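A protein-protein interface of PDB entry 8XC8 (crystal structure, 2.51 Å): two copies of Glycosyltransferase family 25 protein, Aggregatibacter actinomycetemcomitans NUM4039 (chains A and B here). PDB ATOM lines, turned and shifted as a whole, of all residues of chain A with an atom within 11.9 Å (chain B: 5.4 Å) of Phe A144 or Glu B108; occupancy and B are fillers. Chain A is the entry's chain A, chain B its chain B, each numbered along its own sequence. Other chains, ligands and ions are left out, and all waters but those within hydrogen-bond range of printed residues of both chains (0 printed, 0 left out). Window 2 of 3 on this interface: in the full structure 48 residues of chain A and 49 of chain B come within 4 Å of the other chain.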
ATOM      1  N   GLN A 138      22.028 -11.549 -22.822  1.00  0.00           N
ATOM      2  CA  GLN A 138      21.446 -12.367 -21.734  1.00  0.00           C
ATOM      3  C   GLN A 138      20.207 -11.655 -21.201  1.00  0.00           C
ATOM      4  O   GLN A 138      20.216 -10.410 -21.174  1.00  0.00           O
ATOM      5  CB  GLN A 138      22.467 -12.565 -20.608  1.00  0.00           C
ATOM      6  CG  GLN A 138      22.072 -13.638 -19.608  1.00  0.00           C
ATOM      7  CD  GLN A 138      22.098 -15.024 -20.206  1.00  0.00           C
ATOM      8  OE1 GLN A 138      22.198 -15.213 -21.420  1.00  0.00           O
ATOM      9  NE2 GLN A 138      22.003 -16.019 -19.341  1.00  0.00           N
ATOM     10  N   THR A 139      19.203 -12.427 -20.782  1.00  0.00           N
ATOM     11  CA  THR A 139      18.013 -11.941 -20.032  1.00  0.00           C
ATOM     12  C   THR A 139      18.051 -12.465 -18.589  1.00  0.00           C
ATOM     13  O   THR A 139      17.699 -11.686 -17.672  1.00  0.00           O
ATOM     14  CB  THR A 139      16.719 -12.367 -20.731  1.00  0.00           C
ATOM     15  OG1 THR A 139      16.647 -13.791 -20.652  1.00  0.00           O
ATOM     16  CG2 THR A 139      16.652 -11.920 -22.175  1.00  0.00           C
ATOM     17  N   GLN A 140      18.444 -13.731 -18.407  1.00  0.00           N
ATOM     18  CA  GLN A 140      18.366 -14.458 -17.113  1.00  0.00           C
ATOM     19  C   GLN A 140      19.335 -13.806 -16.122  1.00  0.00           C
ATOM     20  O   GLN A 140      18.870 -13.434 -15.027  1.00  0.00           O
ATOM     21  CB  GLN A 140      18.660 -15.948 -17.308  1.00  0.00           C
ATOM     22  CG  GLN A 140      17.732 -16.627 -18.312  1.00  0.00           C
ATOM     23  CD  GLN A 140      18.424 -17.725 -19.087  1.00  0.00           C
ATOM     24  OE1 GLN A 140      19.340 -18.378 -18.587  1.00  0.00           O
ATOM     25  NE2 GLN A 140      17.989 -17.940 -20.321  1.00  0.00           N
ATOM     26  N   ILE A 141      20.608 -13.636 -16.510  1.00  0.00           N
ATOM     27  CA  ILE A 141      21.695 -13.140 -15.610  1.00  0.00           C
ATOM     28  C   ILE A 141      21.807 -11.615 -15.686  1.00  0.00           C
ATOM     29  O   ILE A 141      22.151 -11.032 -16.715  1.00  0.00           O
ATOM     30  CB  ILE A 141      23.048 -13.822 -15.875  1.00  0.00           C
ATOM     31  CG1 ILE A 141      22.937 -15.348 -15.953  1.00  0.00           C
ATOM     32  CG2 ILE A 141      24.050 -13.399 -14.816  1.00  0.00           C
ATOM     33  CD1 ILE A 141      22.418 -15.986 -14.690  1.00  0.00           C
ATOM     34  N   PRO A 142      21.542 -10.930 -14.555  1.00  0.00           N
ATOM     35  CA  PRO A 142      21.444  -9.469 -14.535  1.00  0.00           C
ATOM     36  C   PRO A 142      22.770  -8.744 -14.761  1.00  0.00           C
ATOM     37  O   PRO A 142      23.774  -9.067 -14.132  1.00  0.00           O
ATOM     38  CB  PRO A 142      20.927  -9.164 -13.120  1.00  0.00           C
ATOM     39  CG  PRO A 142      21.359 -10.358 -12.292  1.00  0.00           C
ATOM     40  CD  PRO A 142      21.307 -11.540 -13.237  1.00  0.00           C
ATOM     41  N   PRO A 143      22.805  -7.729 -15.651  1.00  0.00           N
ATOM     42  CA  PRO A 143      23.982  -6.870 -15.830  1.00  0.00           C
ATOM     43  C   PRO A 143      24.472  -6.128 -14.575  1.00  0.00           C
ATOM     44  O   PRO A 143      23.805  -5.205 -14.142  1.00  0.00           O
ATOM     45  CB  PRO A 143      23.502  -5.822 -16.853  1.00  0.00           C
ATOM     46  CG  PRO A 143      22.402  -6.520 -17.614  1.00  0.00           C
ATOM     47  CD  PRO A 143      21.717  -7.378 -16.574  1.00  0.00           C
ATOM     48  N   PHE A 144      25.639  -6.512 -14.046  1.00  0.00           N
ATOM     49  CA  PHE A 144      26.308  -5.834 -12.904  1.00  0.00           C
ATOM     50  C   PHE A 144      27.216  -4.708 -13.406  1.00  0.00           C
ATOM     51  O   PHE A 144      27.946  -4.929 -14.378  1.00  0.00           O
ATOM     52  CB  PHE A 144      27.142  -6.814 -12.078  1.00  0.00           C
ATOM     53  CG  PHE A 144      27.767  -6.191 -10.857  1.00  0.00           C
ATOM     54  CD1 PHE A 144      27.000  -5.469  -9.954  1.00  0.00           C
ATOM     55  CD2 PHE A 144      29.125  -6.313 -10.617  1.00  0.00           C
ATOM     56  CE1 PHE A 144      27.578  -4.888  -8.835  1.00  0.00           C
ATOM     57  CE2 PHE A 144      29.701  -5.741  -9.492  1.00  0.00           C
ATOM     58  CZ  PHE A 144      28.927  -5.028  -8.606  1.00  0.00           C
ATOM     59  N   GLN A 145      27.189  -3.559 -12.723  1.00  0.00           N
ATOM     60  CA  GLN A 145      28.032  -2.367 -13.003  1.00  0.00           C
ATOM     61  C   GLN A 145      27.990  -2.058 -14.505  1.00  0.00           C
ATOM     62  O   GLN A 145      29.074  -1.950 -15.106  1.00  0.00           O
ATOM     63  CB  GLN A 145      29.459  -2.614 -12.508  1.00  0.00           C
ATOM     64  CG  GLN A 145      30.209  -1.346 -12.121  1.00  0.00           C
ATOM     65  CD  GLN A 145      29.970  -0.934 -10.690  1.00  0.00           C
ATOM     66  OE1 GLN A 145      29.009  -1.360 -10.049  1.00  0.00           O
ATOM     67  NE2 GLN A 145      30.858  -0.097 -10.173  1.00  0.00           N
ATOM     68  N   GLN A 146      26.782  -1.942 -15.074  1.00  0.00           N
ATOM     69  CA  GLN A 146      26.486  -1.588 -16.498  1.00  0.00           C
ATOM     70  C   GLN A 146      27.383  -2.385 -17.464  1.00  0.00           C
ATOM     71  O   GLN A 146      27.835  -1.821 -18.487  1.00  0.00           O
ATOM     72  CB  GLN A 146      26.568  -0.070 -16.714  1.00  0.00           C
ATOM     73  CG  GLN A 146      27.960   0.543 -16.579  1.00  0.00           C
ATOM     74  CD  GLN A 146      28.314   0.962 -15.172  1.00  0.00           C
ATOM     75  OE1 GLN A 146      27.467   1.418 -14.406  1.00  0.00           O
ATOM     76  NE2 GLN A 146      29.582   0.819 -14.817  1.00  0.00           N
ATOM     77  N   ARG A 147      27.586  -3.668 -17.163  1.00  0.00           N
ATOM     78  CA  ARG A 147      28.328  -4.636 -18.006  1.00  0.00           C
ATOM     79  C   ARG A 147      27.498  -5.917 -18.118  1.00  0.00           C
ATOM     80  O   ARG A 147      27.216  -6.518 -17.059  1.00  0.00           O
ATOM     81  CB  ARG A 147      29.679  -4.966 -17.372  1.00  0.00           C
ATOM     82  CG  ARG A 147      30.725  -3.866 -17.469  1.00  0.00           C
ATOM     83  CD  ARG A 147      32.033  -4.396 -16.905  1.00  0.00           C
ATOM     84  NE  ARG A 147      33.219  -3.689 -17.360  1.00  0.00           N
ATOM     85  CZ  ARG A 147      33.674  -2.545 -16.855  1.00  0.00           C
ATOM     86  NH1 ARG A 147      33.039  -1.940 -15.863  1.00  0.00           N
ATOM     87  NH2 ARG A 147      34.775  -2.009 -17.356  1.00  0.00           N
ATOM     88  N   ASP A 148      27.129  -6.316 -19.341  1.00  0.00           N
ATOM     89  CA  ASP A 148      26.317  -7.534 -19.602  1.00  0.00           C
ATOM     90  C   ASP A 148      27.182  -8.777 -19.398  1.00  0.00           C
ATOM     91  O   ASP A 148      28.423  -8.668 -19.491  1.00  0.00           O
ATOM     92  CB  ASP A 148      25.726  -7.546 -21.013  1.00  0.00           C
ATOM     93  CG  ASP A 148      24.809  -6.379 -21.311  1.00  0.00           C
ATOM     94  OD1 ASP A 148      24.188  -5.860 -20.355  1.00  0.00           O
ATOM     95  OD2 ASP A 148      24.720  -6.001 -22.503  1.00  0.00           O
ATOM     96  N   ILE A 149      26.526  -9.908 -19.146  1.00  0.00           N
ATOM     97  CA  ILE A 149      27.130 -11.268 -19.181  1.00  0.00           C
ATOM     98  C   ILE A 149      26.600 -11.950 -20.442  1.00  0.00           C
ATOM     99  O   ILE A 149      25.730 -12.824 -20.336  1.00  0.00           O
ATOM    100  CB  ILE A 149      26.812 -12.044 -17.887  1.00  0.00           C
ATOM    101  CG1 ILE A 149      27.354 -11.320 -16.651  1.00  0.00           C
ATOM    102  CG2 ILE A 149      27.340 -13.468 -17.959  1.00  0.00           C
ATOM    103  CD1 ILE A 149      26.423 -10.283 -16.069  1.00  0.00           C
ATOM    104  N   ASP A 150      27.096 -11.528 -21.604  1.00  0.00           N
ATOM    105  CA  ASP A 150      26.727 -12.129 -22.907  1.00  0.00           C
ATOM    106  C   ASP A 150      27.287 -13.550 -22.933  1.00  0.00           C
ATOM    107  O   ASP A 150      28.318 -13.788 -22.274  1.00  0.00           O
ATOM    108  CB  ASP A 150      27.205 -11.262 -24.069  1.00  0.00           C
ATOM    109  CG  ASP A 150      26.712  -9.824 -23.986  1.00  0.00           C
ATOM    110  OD1 ASP A 150      25.494  -9.612 -23.831  1.00  0.00           O
ATOM    111  OD2 ASP A 150      27.552  -8.923 -24.056  1.00  0.00           O
ATOM    112  N   GLN A 230      37.347  -0.776 -26.545  1.00  0.00           N
ATOM    113  CA  GLN A 230      37.580  -1.279 -25.166  1.00  0.00           C
ATOM    114  C   GLN A 230      39.091  -1.421 -24.922  1.00  0.00           C
ATOM    115  O   GLN A 230      39.606  -0.726 -24.015  1.00  0.00           O
ATOM    116  CB  GLN A 230      36.822  -2.597 -24.993  1.00  0.00           C
ATOM    117  CG  GLN A 230      37.060  -3.284 -23.658  1.00  0.00           C
ATOM    118  CD  GLN A 230      36.557  -2.481 -22.483  1.00  0.00           C
ATOM    119  OE1 GLN A 230      35.858  -1.480 -22.631  1.00  0.00           O
ATOM    120  NE2 GLN A 230      36.902  -2.936 -21.291  1.00  0.00           N
ATOM    121  N   TYR B  88      34.605 -21.186  -6.849  1.00  0.00           N
ATOM    122  CA  TYR B  88      35.188 -20.702  -8.122  1.00  0.00           C
ATOM    123  C   TYR B  88      36.601 -20.181  -7.878  1.00  0.00           C
ATOM    124  O   TYR B  88      36.890 -19.717  -6.775  1.00  0.00           O
ATOM    125  CB  TYR B  88      34.352 -19.557  -8.687  1.00  0.00           C
ATOM    126  CG  TYR B  88      34.514 -18.259  -7.943  1.00  0.00           C
ATOM    127  CD1 TYR B  88      33.745 -17.962  -6.832  1.00  0.00           C
ATOM    128  CD2 TYR B  88      35.430 -17.312  -8.362  1.00  0.00           C
ATOM    129  CE1 TYR B  88      33.882 -16.756  -6.158  1.00  0.00           C
ATOM    130  CE2 TYR B  88      35.584 -16.106  -7.694  1.00  0.00           C
ATOM    131  CZ  TYR B  88      34.805 -15.820  -6.589  1.00  0.00           C
ATOM    132  OH  TYR B  88      34.953 -14.620  -5.950  1.00  0.00           O
ATOM    133  N   ASN B 103      38.412  -3.593  -9.437  1.00  0.00           N
ATOM    134  CA  ASN B 103      38.219  -3.828  -7.980  1.00  0.00           C
ATOM    135  C   ASN B 103      36.828  -4.423  -7.737  1.00  0.00           C
ATOM    136  O   ASN B 103      36.783  -5.494  -7.119  1.00  0.00           O
ATOM    137  CB  ASN B 103      38.491  -2.568  -7.155  1.00  0.00           C
ATOM    138  CG  ASN B 103      38.088  -1.273  -7.832  1.00  0.00           C
ATOM    139  OD1 ASN B 103      37.355  -1.279  -8.820  1.00  0.00           O
ATOM    140  ND2 ASN B 103      38.565  -0.154  -7.307  1.00  0.00           N
ATOM    141  N   LYS B 104      35.762  -3.781  -8.231  1.00  0.00           N
ATOM    142  CA  LYS B 104      34.341  -4.146  -7.960  1.00  0.00           C
ATOM    143  C   LYS B 104      34.057  -5.601  -8.369  1.00  0.00           C
ATOM    144  O   LYS B 104      33.149  -6.212  -7.777  1.00  0.00           O
ATOM    145  CB  LYS B 104      33.385  -3.184  -8.683  1.00  0.00           C
ATOM    146  CG  LYS B 104      32.717  -2.122  -7.809  1.00  0.00           C
ATOM    147  CD  LYS B 104      31.676  -2.693  -6.848  1.00  0.00           C
ATOM    148  CE  LYS B 104      30.492  -1.782  -6.588  1.00  0.00           C
ATOM    149  NZ  LYS B 104      30.810  -0.726  -5.599  1.00  0.00           N
ATOM    150  N   PHE B 105      34.790  -6.126  -9.352  1.00  0.00           N
ATOM    151  CA  PHE B 105      34.604  -7.490  -9.915  1.00  0.00           C
ATOM    152  C   PHE B 105      35.530  -8.500  -9.234  1.00  0.00           C
ATOM    153  O   PHE B 105      35.187  -9.684  -9.240  1.00  0.00           O
ATOM    154  CB  PHE B 105      34.886  -7.487 -11.418  1.00  0.00           C
ATOM    155  CG  PHE B 105      33.938  -6.629 -12.213  1.00  0.00           C
ATOM    156  CD1 PHE B 105      32.661  -7.079 -12.507  1.00  0.00           C
ATOM    157  CD2 PHE B 105      34.316  -5.368 -12.646  1.00  0.00           C
ATOM    158  CE1 PHE B 105      31.783  -6.285 -13.225  1.00  0.00           C
ATOM    159  CE2 PHE B 105      33.435  -4.575 -13.365  1.00  0.00           C
ATOM    160  CZ  PHE B 105      32.172  -5.036 -13.653  1.00  0.00           C
ATOM    161  N   LEU B 106      36.665  -8.046  -8.696  1.00  0.00           N
ATOM    162  CA  LEU B 106      37.791  -8.913  -8.252  1.00  0.00           C
ATOM    163  C   LEU B 106      38.000  -8.825  -6.734  1.00  0.00           C
ATOM    164  O   LEU B 106      38.200  -9.889  -6.111  1.00  0.00           O
ATOM    165  CB  LEU B 106      39.041  -8.481  -9.016  1.00  0.00           C
ATOM    166  CG  LEU B 106      38.941  -8.616 -10.534  1.00  0.00           C
ATOM    167  CD1 LEU B 106      40.151  -7.988 -11.211  1.00  0.00           C
ATOM    168  CD2 LEU B 106      38.790 -10.074 -10.942  1.00  0.00           C
ATOM    169  N   ALA B 107      37.980  -7.614  -6.165  1.00  0.00           N
ATOM    170  CA  ALA B 107      38.107  -7.366  -4.707  1.00  0.00           C
ATOM    171  C   ALA B 107      37.080  -8.236  -3.976  1.00  0.00           C
ATOM    172  O   ALA B 107      37.506  -9.097  -3.180  1.00  0.00           O
ATOM    173  CB  ALA B 107      37.926  -5.900  -4.382  1.00  0.00           C
ATOM    174  N   GLU B 108      35.793  -8.042  -4.290  1.00  0.00           N
ATOM    175  CA  GLU B 108      34.644  -8.807  -3.730  1.00  0.00           C
ATOM    176  C   GLU B 108      34.234  -9.900  -4.724  1.00  0.00           C
ATOM    177  O   GLU B 108      34.716  -9.854  -5.876  1.00  0.00           O
ATOM    178  CB  GLU B 108      33.477  -7.859  -3.440  1.00  0.00           C
ATOM    179  CG  GLU B 108      32.802  -7.321  -4.693  1.00  0.00           C
ATOM    180  CD  GLU B 108      31.782  -6.219  -4.475  1.00  0.00           C
ATOM    181  OE1 GLU B 108      31.813  -5.590  -3.399  1.00  0.00           O
ATOM    182  OE2 GLU B 108      30.956  -5.995  -5.386  1.00  0.00           O
ATOM    183  N   GLY B 109      33.374 -10.829  -4.291  1.00  0.00           N
ATOM    184  CA  GLY B 109      32.769 -11.868  -5.145  1.00  0.00           C
ATOM    185  C   GLY B 109      31.332 -12.182  -4.752  1.00  0.00           C
ATOM    186  O   GLY B 109      30.954 -13.370  -4.825  1.00  0.00           O
ATOM    187  N   ASP B 110      30.537 -11.160  -4.414  1.00  0.00           N
ATOM    188  CA  ASP B 110      29.122 -11.323  -3.980  1.00  0.00           C
ATOM    189  C   ASP B 110      28.214 -11.261  -5.215  1.00  0.00           C
ATOM    190  O   ASP B 110      27.405 -12.196  -5.398  1.00  0.00           O
ATOM    191  CB  ASP B 110      28.751 -10.288  -2.917  1.00  0.00           C
ATOM    192  CG  ASP B 110      29.610 -10.374  -1.667  1.00  0.00           C
ATOM    193  OD1 ASP B 110      30.797  -9.984  -1.736  1.00  0.00           O
ATOM    194  OD2 ASP B 110      29.088 -10.841  -0.635  1.00  0.00           O
ATOM    195  N   TRP B 111      28.377 -10.214  -6.036  1.00  0.00           N
ATOM    196  CA  TRP B 111      27.751 -10.055  -7.380  1.00  0.00           C
ATOM    197  C   TRP B 111      27.806 -11.384  -8.147  1.00  0.00           C
ATOM    198  O   TRP B 111      26.902 -11.639  -8.975  1.00  0.00           O
ATOM    199  CB  TRP B 111      28.462  -8.955  -8.178  1.00  0.00           C
ATOM    200  CG  TRP B 111      29.857  -9.324  -8.582  1.00  0.00           C
ATOM    201  CD1 TRP B 111      30.971  -9.292  -7.796  1.00  0.00           C
ATOM    202  CD2 TRP B 111      30.295  -9.807  -9.868  1.00  0.00           C
ATOM    203  NE1 TRP B 111      32.070  -9.695  -8.508  1.00  0.00           N
ATOM    204  CE2 TRP B 111      31.687 -10.023  -9.778  1.00  0.00           C
ATOM    205  CE3 TRP B 111      29.658 -10.059 -11.090  1.00  0.00           C
ATOM    206  CZ2 TRP B 111      32.437 -10.492 -10.856  1.00  0.00           C
ATOM    207  CZ3 TRP B 111      30.402 -10.519 -12.154  1.00  0.00           C
ATOM    208  CH2 TRP B 111      31.774 -10.729 -12.037  1.00  0.00           C
ATOM    209  N   ARG B 115      24.449 -14.316  -8.845  1.00  0.00           N
ATOM    210  CA  ARG B 115      24.172 -14.439 -10.305  1.00  0.00           C
ATOM    211  C   ARG B 115      24.338 -15.880 -10.809  1.00  0.00           C
ATOM    212  O   ARG B 115      23.785 -16.169 -11.887  1.00  0.00           O
ATOM    213  CB  ARG B 115      25.057 -13.458 -11.080  1.00  0.00           C
ATOM    214  CG  ARG B 115      24.545 -12.027 -11.012  1.00  0.00           C
ATOM    215  CD  ARG B 115      25.412 -11.002 -11.708  1.00  0.00           C
ATOM    216  NE  ARG B 115      24.807  -9.674 -11.672  1.00  0.00           N
ATOM    217  CZ  ARG B 115      24.764  -8.869 -10.604  1.00  0.00           C
ATOM    218  NH1 ARG B 115      25.297  -9.241  -9.452  1.00  0.00           N
ATOM    219  NH2 ARG B 115      24.186  -7.681 -10.696  1.00  0.00           N
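Of the 11 printed residues of chain B, 5 touch a printed residue of chain A.
Printed residues of chain A that touch a printed residue of chain B: Ile A141, Pro A142, Phe A144, Gln A145 and Arg A147.
Hydrophobic or aromatic side chains of chain A that line the printed part of chain B: Ile A141, Pro A142 and Phe A144.
Among the printed residues, 10 pairs touch across the chains.
Among the printed residues, pairs that only touch across the chains: Ile A141 with Arg B115, Arg A147 with Phe B105, Phe A144 with Arg B115, Gln A145 with Lys B104, Phe A144 with Trp B111, Phe A144 with Phe B105, Gln A145 with Phe B105, Phe A144 with Lys B104 and Phe A144 with Glu B108.
The guanidinium group (NE) of Arg B115 sits at hydrogen-bond distance from the backbone carbonyl oxygen (O) of Pro A142 (2.7 Å).
No position is printed for both chains.
The indole nitrogen (NE1) of Trp B111 is in hydrogen-bond range of the backbone carbonyl oxygen (O) of Phe B105, at 3.2 Å.
The guanidinium group (NH1) of Arg B115 lies within hydrogen-bond range of the backbone carbonyl oxygen (O) of Trp B111 (2.9 Å).
Of the printed residues of chain B, Ile A141 touches Arg B115.
Of the printed residues of chain B, Pro A142 touches Arg B115 (2.7 Å).
Printed residues of chain B within 4 Å of Phe A144: Lys B104, Phe B105, Glu B108, Trp B111 and Arg B115.
Of the printed residues of chain B, Arg A147 touches Phe B105 (3.3 Å).
Asp A150 touches none of the printed residues of chain B.
Lys B104 touches two residues of chain A.
Phe B105 touches just these residues of chain A: Phe A144 (3.7 Å), Gln A145 (3.8 Å) and Arg A147 (3.3 Å).
No residue of chain A comes within 4 Å of Leu B106.
Glu B108 touches one residue of chain A.
No residue of chain A comes within 4 Å of Asp B110.
Of chain A, only Phe A144 comes within 4 Å of Trp B111.
Of the printed residues of chain A, Arg B115 touches Ile A141, Pro A142 and Phe A144.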
